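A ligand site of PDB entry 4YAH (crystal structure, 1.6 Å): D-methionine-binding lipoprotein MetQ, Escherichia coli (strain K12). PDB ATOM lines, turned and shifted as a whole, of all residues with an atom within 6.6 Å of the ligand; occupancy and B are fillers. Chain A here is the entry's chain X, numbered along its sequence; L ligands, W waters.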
ATOM      1  N   GLU A  42      13.725 -19.226   5.118  1.00  0.00           N
ATOM      2  CA  GLU A  42      13.128 -20.492   5.549  1.00  0.00           C
ATOM      3  C   GLU A  42      12.222 -21.039   4.441  1.00  0.00           C
ATOM      4  O   GLU A  42      12.164 -22.249   4.214  1.00  0.00           O
ATOM      5  CB  GLU A  42      12.347 -20.346   6.862  1.00  0.00           C
ATOM      6  CG  GLU A  42      13.288 -20.126   8.076  1.00  0.00           C
ATOM      7  CD  GLU A  42      12.605 -20.135   9.429  1.00  0.00           C
ATOM      8  OE1 GLU A  42      13.220 -19.628  10.400  1.00  0.00           O
ATOM      9  OE2 GLU A  42      11.486 -20.652   9.559  1.00  0.00           O
ATOM     10  N   TYR A  69       4.390 -15.665  13.673  1.00  0.00           N
ATOM     11  CA  TYR A  69       4.547 -16.891  14.416  1.00  0.00           C
ATOM     12  C   TYR A  69       3.236 -17.380  15.056  1.00  0.00           C
ATOM     13  O   TYR A  69       3.242 -18.402  15.752  1.00  0.00           O
ATOM     14  CB  TYR A  69       5.579 -16.682  15.513  1.00  0.00           C
ATOM     15  CG  TYR A  69       7.039 -16.668  15.081  1.00  0.00           C
ATOM     16  CD1 TYR A  69       7.456 -17.248  13.896  1.00  0.00           C
ATOM     17  CD2 TYR A  69       8.005 -16.138  15.912  1.00  0.00           C
ATOM     18  CE1 TYR A  69       8.787 -17.284  13.559  1.00  0.00           C
ATOM     19  CE2 TYR A  69       9.336 -16.165  15.586  1.00  0.00           C
ATOM     20  CZ  TYR A  69       9.727 -16.737  14.432  1.00  0.00           C
ATOM     21  OH  TYR A  69      11.068 -16.745  14.137  1.00  0.00           O
ATOM     22  N   PHE A  86       8.216 -24.241  11.453  1.00  0.00           N
ATOM     23  CA  PHE A  86       8.679 -22.897  11.805  1.00  0.00           C
ATOM     24  C   PHE A  86       9.020 -22.637  13.263  1.00  0.00           C
ATOM     25  O   PHE A  86       9.521 -21.559  13.576  1.00  0.00           O
ATOM     26  CB  PHE A  86       7.600 -21.862  11.410  1.00  0.00           C
ATOM     27  CG  PHE A  86       6.511 -21.702  12.438  1.00  0.00           C
ATOM     28  CD1 PHE A  86       6.551 -20.655  13.335  1.00  0.00           C
ATOM     29  CD2 PHE A  86       5.468 -22.619  12.537  1.00  0.00           C
ATOM     30  CE1 PHE A  86       5.577 -20.502  14.302  1.00  0.00           C
ATOM     31  CE2 PHE A  86       4.487 -22.472  13.500  1.00  0.00           C
ATOM     32  CZ  PHE A  86       4.536 -21.418  14.372  1.00  0.00           C
ATOM     33  N   GLN A  87       8.742 -23.585  14.162  1.00  0.00           N
ATOM     34  CA  GLN A  87       8.847 -23.322  15.598  1.00  0.00           C
ATOM     35  C   GLN A  87       9.721 -24.330  16.329  1.00  0.00           C
ATOM     36  O   GLN A  87       9.902 -25.458  15.869  1.00  0.00           O
ATOM     37  CB  GLN A  87       7.444 -23.279  16.221  1.00  0.00           C
ATOM     38  CG  GLN A  87       6.790 -24.643  16.374  1.00  0.00           C
ATOM     39  CD  GLN A  87       5.276 -24.576  16.506  1.00  0.00           C
ATOM     40  OE1 GLN A  87       4.745 -24.000  17.471  1.00  0.00           O
ATOM     41  NE2 GLN A  87       4.576 -25.173  15.544  1.00  0.00           N
ATOM     42  N   HIS A  88      10.295 -23.915  17.455  1.00  0.00           N
ATOM     43  CA  HIS A  88      11.029 -24.832  18.314  1.00  0.00           C
ATOM     44  C   HIS A  88      10.095 -25.363  19.412  1.00  0.00           C
ATOM     45  O   HIS A  88       8.947 -24.903  19.522  1.00  0.00           O
ATOM     46  CB  HIS A  88      12.298 -24.166  18.919  1.00  0.00           C
ATOM     47  CG  HIS A  88      12.104 -22.803  19.498  1.00  0.00           C
ATOM     48  ND1 HIS A  88      11.239 -22.534  20.549  1.00  0.00           N
ATOM     49  CD2 HIS A  88      12.700 -21.624  19.198  1.00  0.00           C
ATOM     50  CE1 HIS A  88      11.305 -21.251  20.852  1.00  0.00           C
ATOM     51  NE2 HIS A  88      12.183 -20.671  20.049  1.00  0.00           N
ATOM     52  N   TYR A  91       8.497 -23.046  22.156  1.00  0.00           N
ATOM     53  CA  TYR A  91       7.427 -22.243  21.572  1.00  0.00           C
ATOM     54  C   TYR A  91       6.158 -23.084  21.425  1.00  0.00           C
ATOM     55  O   TYR A  91       5.065 -22.633  21.777  1.00  0.00           O
ATOM     56  CB  TYR A  91       7.838 -21.704  20.212  1.00  0.00           C
ATOM     57  CG  TYR A  91       6.834 -20.734  19.664  1.00  0.00           C
ATOM     58  CD1 TYR A  91       6.920 -19.385  19.984  1.00  0.00           C
ATOM     59  CD2 TYR A  91       5.786 -21.147  18.849  1.00  0.00           C
ATOM     60  CE1 TYR A  91       6.004 -18.458  19.495  1.00  0.00           C
ATOM     61  CE2 TYR A  91       4.872 -20.236  18.356  1.00  0.00           C
ATOM     62  CZ  TYR A  91       4.981 -18.887  18.685  1.00  0.00           C
ATOM     63  OH  TYR A  91       4.091 -17.955  18.221  1.00  0.00           O
ATOM     64  N   LEU A  92       6.321 -24.278  20.871  1.00  0.00           N
ATOM     65  CA  LEU A  92       5.199 -25.200  20.693  1.00  0.00           C
ATOM     66  C   LEU A  92       4.495 -25.442  22.033  1.00  0.00           C
ATOM     67  O   LEU A  92       3.275 -25.294  22.137  1.00  0.00           O
ATOM     68  CB  LEU A  92       5.680 -26.516  20.098  1.00  0.00           C
ATOM     69  CG  LEU A  92       4.621 -27.612  19.998  1.00  0.00           C
ATOM     70  CD1 LEU A  92       3.469 -27.116  19.119  1.00  0.00           C
ATOM     71  CD2 LEU A  92       5.250 -28.867  19.433  1.00  0.00           C
ATOM     72  N   PHE A 110      16.195 -27.551  11.856  1.00  0.00           N
ATOM     73  CA  PHE A 110      17.488 -26.949  12.221  1.00  0.00           C
ATOM     74  C   PHE A 110      17.437 -26.175  13.533  1.00  0.00           C
ATOM     75  O   PHE A 110      16.382 -25.661  13.923  1.00  0.00           O
ATOM     76  CB  PHE A 110      17.989 -26.006  11.122  1.00  0.00           C
ATOM     77  CG  PHE A 110      18.094 -26.653   9.777  1.00  0.00           C
ATOM     78  CD1 PHE A 110      19.219 -27.402   9.444  1.00  0.00           C
ATOM     79  CD2 PHE A 110      17.076 -26.527   8.850  1.00  0.00           C
ATOM     80  CE1 PHE A 110      19.304 -28.014   8.202  1.00  0.00           C
ATOM     81  CE2 PHE A 110      17.157 -27.152   7.611  1.00  0.00           C
ATOM     82  CZ  PHE A 110      18.279 -27.885   7.281  1.00  0.00           C
ATOM     83  N   VAL A 111      18.582 -26.093  14.204  1.00  0.00           N
ATOM     84  CA  VAL A 111      18.778 -25.075  15.227  1.00  0.00           C
ATOM     85  C   VAL A 111      19.280 -23.819  14.504  1.00  0.00           C
ATOM     86  O   VAL A 111      20.135 -23.911  13.626  1.00  0.00           O
ATOM     87  CB  VAL A 111      19.816 -25.485  16.296  1.00  0.00           C
ATOM     88  CG1 VAL A 111      19.906 -24.424  17.385  1.00  0.00           C
ATOM     89  CG2 VAL A 111      19.507 -26.843  16.892  1.00  0.00           C
ATOM     90  N   TYR A 112      18.730 -22.655  14.872  1.00  0.00           N
ATOM     91  CA  TYR A 112      19.089 -21.365  14.292  1.00  0.00           C
ATOM     92  C   TYR A 112      19.598 -20.476  15.418  1.00  0.00           C
ATOM     93  O   TYR A 112      18.821 -19.736  16.012  1.00  0.00           O
ATOM     94  CB  TYR A 112      17.893 -20.721  13.614  1.00  0.00           C
ATOM     95  CG  TYR A 112      17.375 -21.435  12.392  1.00  0.00           C
ATOM     96  CD1 TYR A 112      18.103 -21.445  11.212  1.00  0.00           C
ATOM     97  CD2 TYR A 112      16.139 -22.046  12.417  1.00  0.00           C
ATOM     98  CE1 TYR A 112      17.606 -22.073  10.074  1.00  0.00           C
ATOM     99  CE2 TYR A 112      15.628 -22.677  11.281  1.00  0.00           C
ATOM    100  CZ  TYR A 112      16.374 -22.689  10.123  1.00  0.00           C
ATOM    101  OH  TYR A 112      15.902 -23.286   8.994  1.00  0.00           O
ATOM    102  N   PRO A 113      20.902 -20.580  15.749  1.00  0.00           N
ATOM    103  CA  PRO A 113      21.375 -19.823  16.912  1.00  0.00           C
ATOM    104  C   PRO A 113      21.109 -18.331  16.725  1.00  0.00           C
ATOM    105  O   PRO A 113      21.391 -17.767  15.674  1.00  0.00           O
ATOM    106  CB  PRO A 113      22.869 -20.159  16.965  1.00  0.00           C
ATOM    107  CG  PRO A 113      22.965 -21.535  16.302  1.00  0.00           C
ATOM    108  CD  PRO A 113      21.959 -21.417  15.168  1.00  0.00           C
ATOM    109  N   ILE A 114      20.494 -17.733  17.728  1.00  0.00           N
ATOM    110  CA  ILE A 114      19.999 -16.378  17.593  1.00  0.00           C
ATOM    111  C   ILE A 114      21.105 -15.379  17.932  1.00  0.00           C
ATOM    112  O   ILE A 114      21.996 -15.665  18.718  1.00  0.00           O
ATOM    113  CB  ILE A 114      18.770 -16.156  18.494  1.00  0.00           C
ATOM    114  CG1 ILE A 114      17.956 -14.966  18.010  1.00  0.00           C
ATOM    115  CG2 ILE A 114      19.163 -16.065  19.966  1.00  0.00           C
ATOM    116  CD1 ILE A 114      16.587 -14.873  18.673  1.00  0.00           C
ATOM    117  N   ASP A 138       7.181 -12.763  22.573  1.00  0.00           N
ATOM    118  CA  ASP A 138       6.513 -14.018  22.935  1.00  0.00           C
ATOM    119  C   ASP A 138       7.331 -14.686  24.044  1.00  0.00           C
ATOM    120  O   ASP A 138       8.554 -14.537  24.088  1.00  0.00           O
ATOM    121  CB  ASP A 138       6.361 -14.923  21.717  1.00  0.00           C
ATOM    122  CG  ASP A 138       7.687 -15.309  21.118  1.00  0.00           C
ATOM    123  OD1 ASP A 138       8.272 -14.464  20.395  1.00  0.00           O
ATOM    124  OD2 ASP A 138       8.158 -16.436  21.426  1.00  0.00           O
ATOM    125  N   THR A 140       8.730 -17.535  25.088  1.00  0.00           N
ATOM    126  CA  THR A 140       9.925 -18.362  25.022  1.00  0.00           C
ATOM    127  C   THR A 140      11.058 -17.657  24.266  1.00  0.00           C
ATOM    128  O   THR A 140      12.224 -17.831  24.615  1.00  0.00           O
ATOM    129  CB  THR A 140       9.654 -19.732  24.383  1.00  0.00           C
ATOM    130  OG1 THR A 140       9.213 -19.600  23.030  1.00  0.00           O
ATOM    131  CG2 THR A 140       8.613 -20.469  25.180  1.00  0.00           C
ATOM    132  N   ASN A 141      10.747 -16.842  23.261  1.00  0.00           N
ATOM    133  CA  ASN A 141      11.852 -16.177  22.561  1.00  0.00           C
ATOM    134  C   ASN A 141      12.283 -14.943  23.330  1.00  0.00           C
ATOM    135  O   ASN A 141      13.457 -14.563  23.262  1.00  0.00           O
ATOM    136  CB  ASN A 141      11.462 -15.875  21.116  1.00  0.00           C
ATOM    137  CG  ASN A 141      11.457 -17.130  20.270  1.00  0.00           C
ATOM    138  OD1 ASN A 141      12.498 -17.717  19.987  1.00  0.00           O
ATOM    139  ND2 ASN A 141      10.269 -17.562  19.871  1.00  0.00           N
ATOM    140  N   ARG A 144      14.524 -16.538  25.922  1.00  0.00           N
ATOM    141  CA  ARG A 144      15.736 -16.878  25.201  1.00  0.00           C
ATOM    142  C   ARG A 144      16.668 -15.671  24.982  1.00  0.00           C
ATOM    143  O   ARG A 144      17.885 -15.783  25.126  1.00  0.00           O
ATOM    144  CB  ARG A 144      15.325 -17.470  23.863  1.00  0.00           C
ATOM    145  CG  ARG A 144      16.441 -17.817  22.943  1.00  0.00           C
ATOM    146  CD  ARG A 144      15.878 -18.267  21.627  1.00  0.00           C
ATOM    147  NE  ARG A 144      16.881 -18.874  20.769  1.00  0.00           N
ATOM    148  CZ  ARG A 144      16.646 -19.293  19.540  1.00  0.00           C
ATOM    149  NH1 ARG A 144      15.437 -19.146  18.982  1.00  0.00           N
ATOM    150  NH2 ARG A 144      17.630 -19.853  18.842  1.00  0.00           N
ATOM    151  N   ILE A 201      17.290 -10.815  17.243  1.00  0.00           N
ATOM    152  CA  ILE A 201      16.388 -11.081  16.131  1.00  0.00           C
ATOM    153  C   ILE A 201      16.483 -12.541  15.693  1.00  0.00           C
ATOM    154  O   ILE A 201      17.565 -13.037  15.402  1.00  0.00           O
ATOM    155  CB  ILE A 201      16.706 -10.206  14.903  1.00  0.00           C
ATOM    156  CG1 ILE A 201      16.884  -8.748  15.323  1.00  0.00           C
ATOM    157  CG2 ILE A 201      15.611 -10.335  13.866  1.00  0.00           C
ATOM    158  CD1 ILE A 201      17.158  -7.758  14.170  1.00  0.00           C
ATOM    159  N   ASN A 202      15.338 -13.217  15.633  1.00  0.00           N
ATOM    160  CA  ASN A 202      15.319 -14.556  15.061  1.00  0.00           C
ATOM    161  C   ASN A 202      15.901 -14.551  13.662  1.00  0.00           C
ATOM    162  O   ASN A 202      15.594 -13.696  12.862  1.00  0.00           O
ATOM    163  CB  ASN A 202      13.902 -15.120  15.002  1.00  0.00           C
ATOM    164  CG  ASN A 202      13.208 -15.122  16.339  1.00  0.00           C
ATOM    165  OD1 ASN A 202      12.561 -14.142  16.725  1.00  0.00           O
ATOM    166  ND2 ASN A 202      13.308 -16.239  17.066  1.00  0.00           N
ATOM    167  N   THR A 203      16.697 -15.559  13.361  1.00  0.00           N
ATOM    168  CA  THR A 203      17.312 -15.632  12.046  1.00  0.00           C
ATOM    169  C   THR A 203      16.273 -15.690  10.932  1.00  0.00           C
ATOM    170  O   THR A 203      16.557 -15.228   9.832  1.00  0.00           O
ATOM    171  CB  THR A 203      18.244 -16.829  11.992  1.00  0.00           C
ATOM    172  OG1 THR A 203      19.180 -16.712  13.069  1.00  0.00           O
ATOM    173  CG2 THR A 203      19.002 -16.874  10.689  1.00  0.00           C
ATOM    174  N   THR A 204      15.073 -16.202  11.243  1.00  0.00           N
ATOM    175  CA  THR A 204      13.899 -16.151  10.349  1.00  0.00           C
ATOM    176  C   THR A 204      13.744 -14.771   9.693  1.00  0.00           C
ATOM    177  O   THR A 204      13.638 -14.646   8.474  1.00  0.00           O
ATOM    178  CB  THR A 204      12.584 -16.407  11.118  1.00  0.00           C
ATOM    179  OG1 THR A 204      12.692 -17.588  11.925  1.00  0.00           O
ATOM    180  CG2 THR A 204      11.422 -16.543  10.156  1.00  0.00           C
ATOM    181  N   TYR A 227      16.618 -25.115  21.209  1.00  0.00           N
ATOM    182  CA  TYR A 227      15.735 -24.440  20.249  1.00  0.00           C
ATOM    183  C   TYR A 227      15.739 -25.027  18.837  1.00  0.00           C
ATOM    184  O   TYR A 227      15.455 -24.337  17.871  1.00  0.00           O
ATOM    185  CB  TYR A 227      16.100 -22.936  20.206  1.00  0.00           C
ATOM    186  CG  TYR A 227      15.977 -22.295  21.566  1.00  0.00           C
ATOM    187  CD1 TYR A 227      14.738 -22.123  22.164  1.00  0.00           C
ATOM    188  CD2 TYR A 227      17.090 -21.859  22.263  1.00  0.00           C
ATOM    189  CE1 TYR A 227      14.610 -21.565  23.408  1.00  0.00           C
ATOM    190  CE2 TYR A 227      16.983 -21.293  23.509  1.00  0.00           C
ATOM    191  CZ  TYR A 227      15.746 -21.130  24.067  1.00  0.00           C
ATOM    192  OH  TYR A 227      15.646 -20.557  25.317  1.00  0.00           O
ATOM    193  N   VAL A 228      15.980 -26.331  18.708  1.00  0.00           N
ATOM    194  CA  VAL A 228      15.862 -26.961  17.396  1.00  0.00           C
ATOM    195  C   VAL A 228      14.421 -26.748  16.912  1.00  0.00           C
ATOM    196  O   VAL A 228      13.471 -26.889  17.680  1.00  0.00           O
ATOM    197  CB  VAL A 228      16.240 -28.457  17.421  1.00  0.00           C
ATOM    198  CG1 VAL A 228      15.231 -29.278  18.238  1.00  0.00           C
ATOM    199  CG2 VAL A 228      16.407 -28.971  16.017  1.00  0.00           C
ATOM    200  N   ASN A 229      14.276 -26.350  15.649  1.00  0.00           N
ATOM    201  CA  ASN A 229      12.959 -26.147  15.068  1.00  0.00           C
ATOM    202  C   ASN A 229      12.357 -27.500  14.694  1.00  0.00           C
ATOM    203  O   ASN A 229      13.061 -28.511  14.629  1.00  0.00           O
ATOM    204  CB  ASN A 229      13.050 -25.224  13.833  1.00  0.00           C
ATOM    205  CG  ASN A 229      13.226 -23.751  14.209  1.00  0.00           C
ATOM    206  OD1 ASN A 229      12.841 -22.877  13.440  1.00  0.00           O
ATOM    207  ND2 ASN A 229      13.851 -23.477  15.362  1.00  0.00           N
HETATM  208  N1  LIG L   1      13.086 -20.040  13.547  1.00  0.00           N
HETATM  209  C1  LIG L   1      12.865 -19.456  14.864  1.00  0.00           C
HETATM  210  C2  LIG L   1      14.103 -19.631  15.711  1.00  0.00           C
HETATM  211  O1  LIG L   1      14.613 -20.754  15.772  1.00  0.00           O
HETATM  212  C3  LIG L   1      11.661 -20.103  15.556  1.00  0.00           C
HETATM  213  C4  LIG L   1      11.240 -19.429  16.857  1.00  0.00           C
HETATM  214  S1  LIG L   1       9.832 -20.208  17.673  1.00  0.00           S
HETATM  215  C5  LIG L   1       8.503 -19.674  16.594  1.00  0.00           C
HETATM  216  O2  LIG L   1      14.580 -18.671  16.340  1.00  0.00           O
HETATM  217  O   HOH W   1      15.339 -18.579  13.048  1.00  0.00           O
HETATM  218  O   HOH W   2      16.946 -17.737  15.366  1.00  0.00           O
HETATM  219  O   HOH W   3      16.731 -22.037  16.869  1.00  0.00           O
HETATM  220  O   HOH W   4      10.657 -19.763  12.030  1.00  0.00           O
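An oxygen (O2) of the ligand is in salt-bridge range of the guanidinium group (NH1) of Arg 144 (2.8 Å). ND2 of Asn 202 is in hydrogen-bond range of O2 of the ligand (2.8 Å). OD1 of Asn 229 is in hydrogen-bond range of N1 of the ligand. The side-chain hydroxyl of Thr 204 is in hydrogen-bond range of a nitrogen (N1) of the ligand (3.0 Å). OE1 of Glu 42 lies within salt-bridge range of N1 of the ligand (3.2 Å). A sulfur (S1) of the ligand sits close to the backbone NH (N) of His 88. NE2 of His 88 lies close to S1 of the ligand. The side-chain amide nitrogen (ND2) of Asn 141 sits close to a sulfur (S1) of the ligand, 3.5 Å away.
NH2 of Arg 144 sits at hydrogen-bond distance from O of Tyr 112 (3.1 Å). ND2 of Asn 202 lies within hydrogen-bond range of OD1 of Asn 141. The backbone carbonyl oxygen (O) of Tyr 227 lies within hydrogen-bond range of the side-chain amide nitrogen (ND2) of Asn 229 (3.1 Å). O of Phe 110 sits at hydrogen-bond distance from N of Asn 229, at 2.8 Å. OE1 of Glu 42 lies within hydrogen-bond range of OG1 of Thr 204, 2.6 Å away. O of Tyr 69 is in hydrogen-bond range of OH of Tyr 91 (2.6 Å). The side-chain amide oxygen (OD1) of Asn 141 is in hydrogen-bond range of a ring nitrogen (NE2) of His 88. The side-chain carboxylate of Asp 138 lies within hydrogen-bond range of the side-chain amide nitrogen of Asn 141 (2.9 Å).
OH of Tyr 69 touches C1 of the ligand, 3.3 Å away. O of Phe 86 touches C3 of the ligand (3.3 Å). CB of Gln 87 touches C5 of the ligand, at 3.8 Å. Tyr 91 touches the ligand. Tyr 112 touches the ligand. Hydrophobic or aromatic side chains within 4 Å of the ligand: Tyr 69, Phe 86, His 88, Tyr 91 and Tyr 112. 12 residues have an atom within 4 Å of the ligand: Glu 42, Tyr 69, Phe 86, Gln 87, His 88, Tyr 91, Tyr 112, Asn 141, Arg 144, Asn 202, Thr 204 and Asn 229.
Water W3 lies within hydrogen-bond range of an oxygen (O1) of the ligand, the backbone carbonyl oxygen of Tyr 227, the backbone NH of Tyr 112 and the guanidinium group of Arg 144. Water W2 lies within hydrogen-bond range of O2 of the ligand (2.7 Å), O of Tyr 112 (2.8 Å) and N of Thr 203 (3.0 Å). Water W1 lies within hydrogen-bond range of N1 of the ligand (2.7 Å), N of Thr 204 (3.0 Å) and N of Thr 203 (3.3 Å). Water W4 lies within hydrogen-bond range of the backbone carbonyl oxygen of Phe 86, the side-chain carboxylate of Glu 42, a nitrogen (N1) of the ligand and the side-chain hydroxyl of Thr 204.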
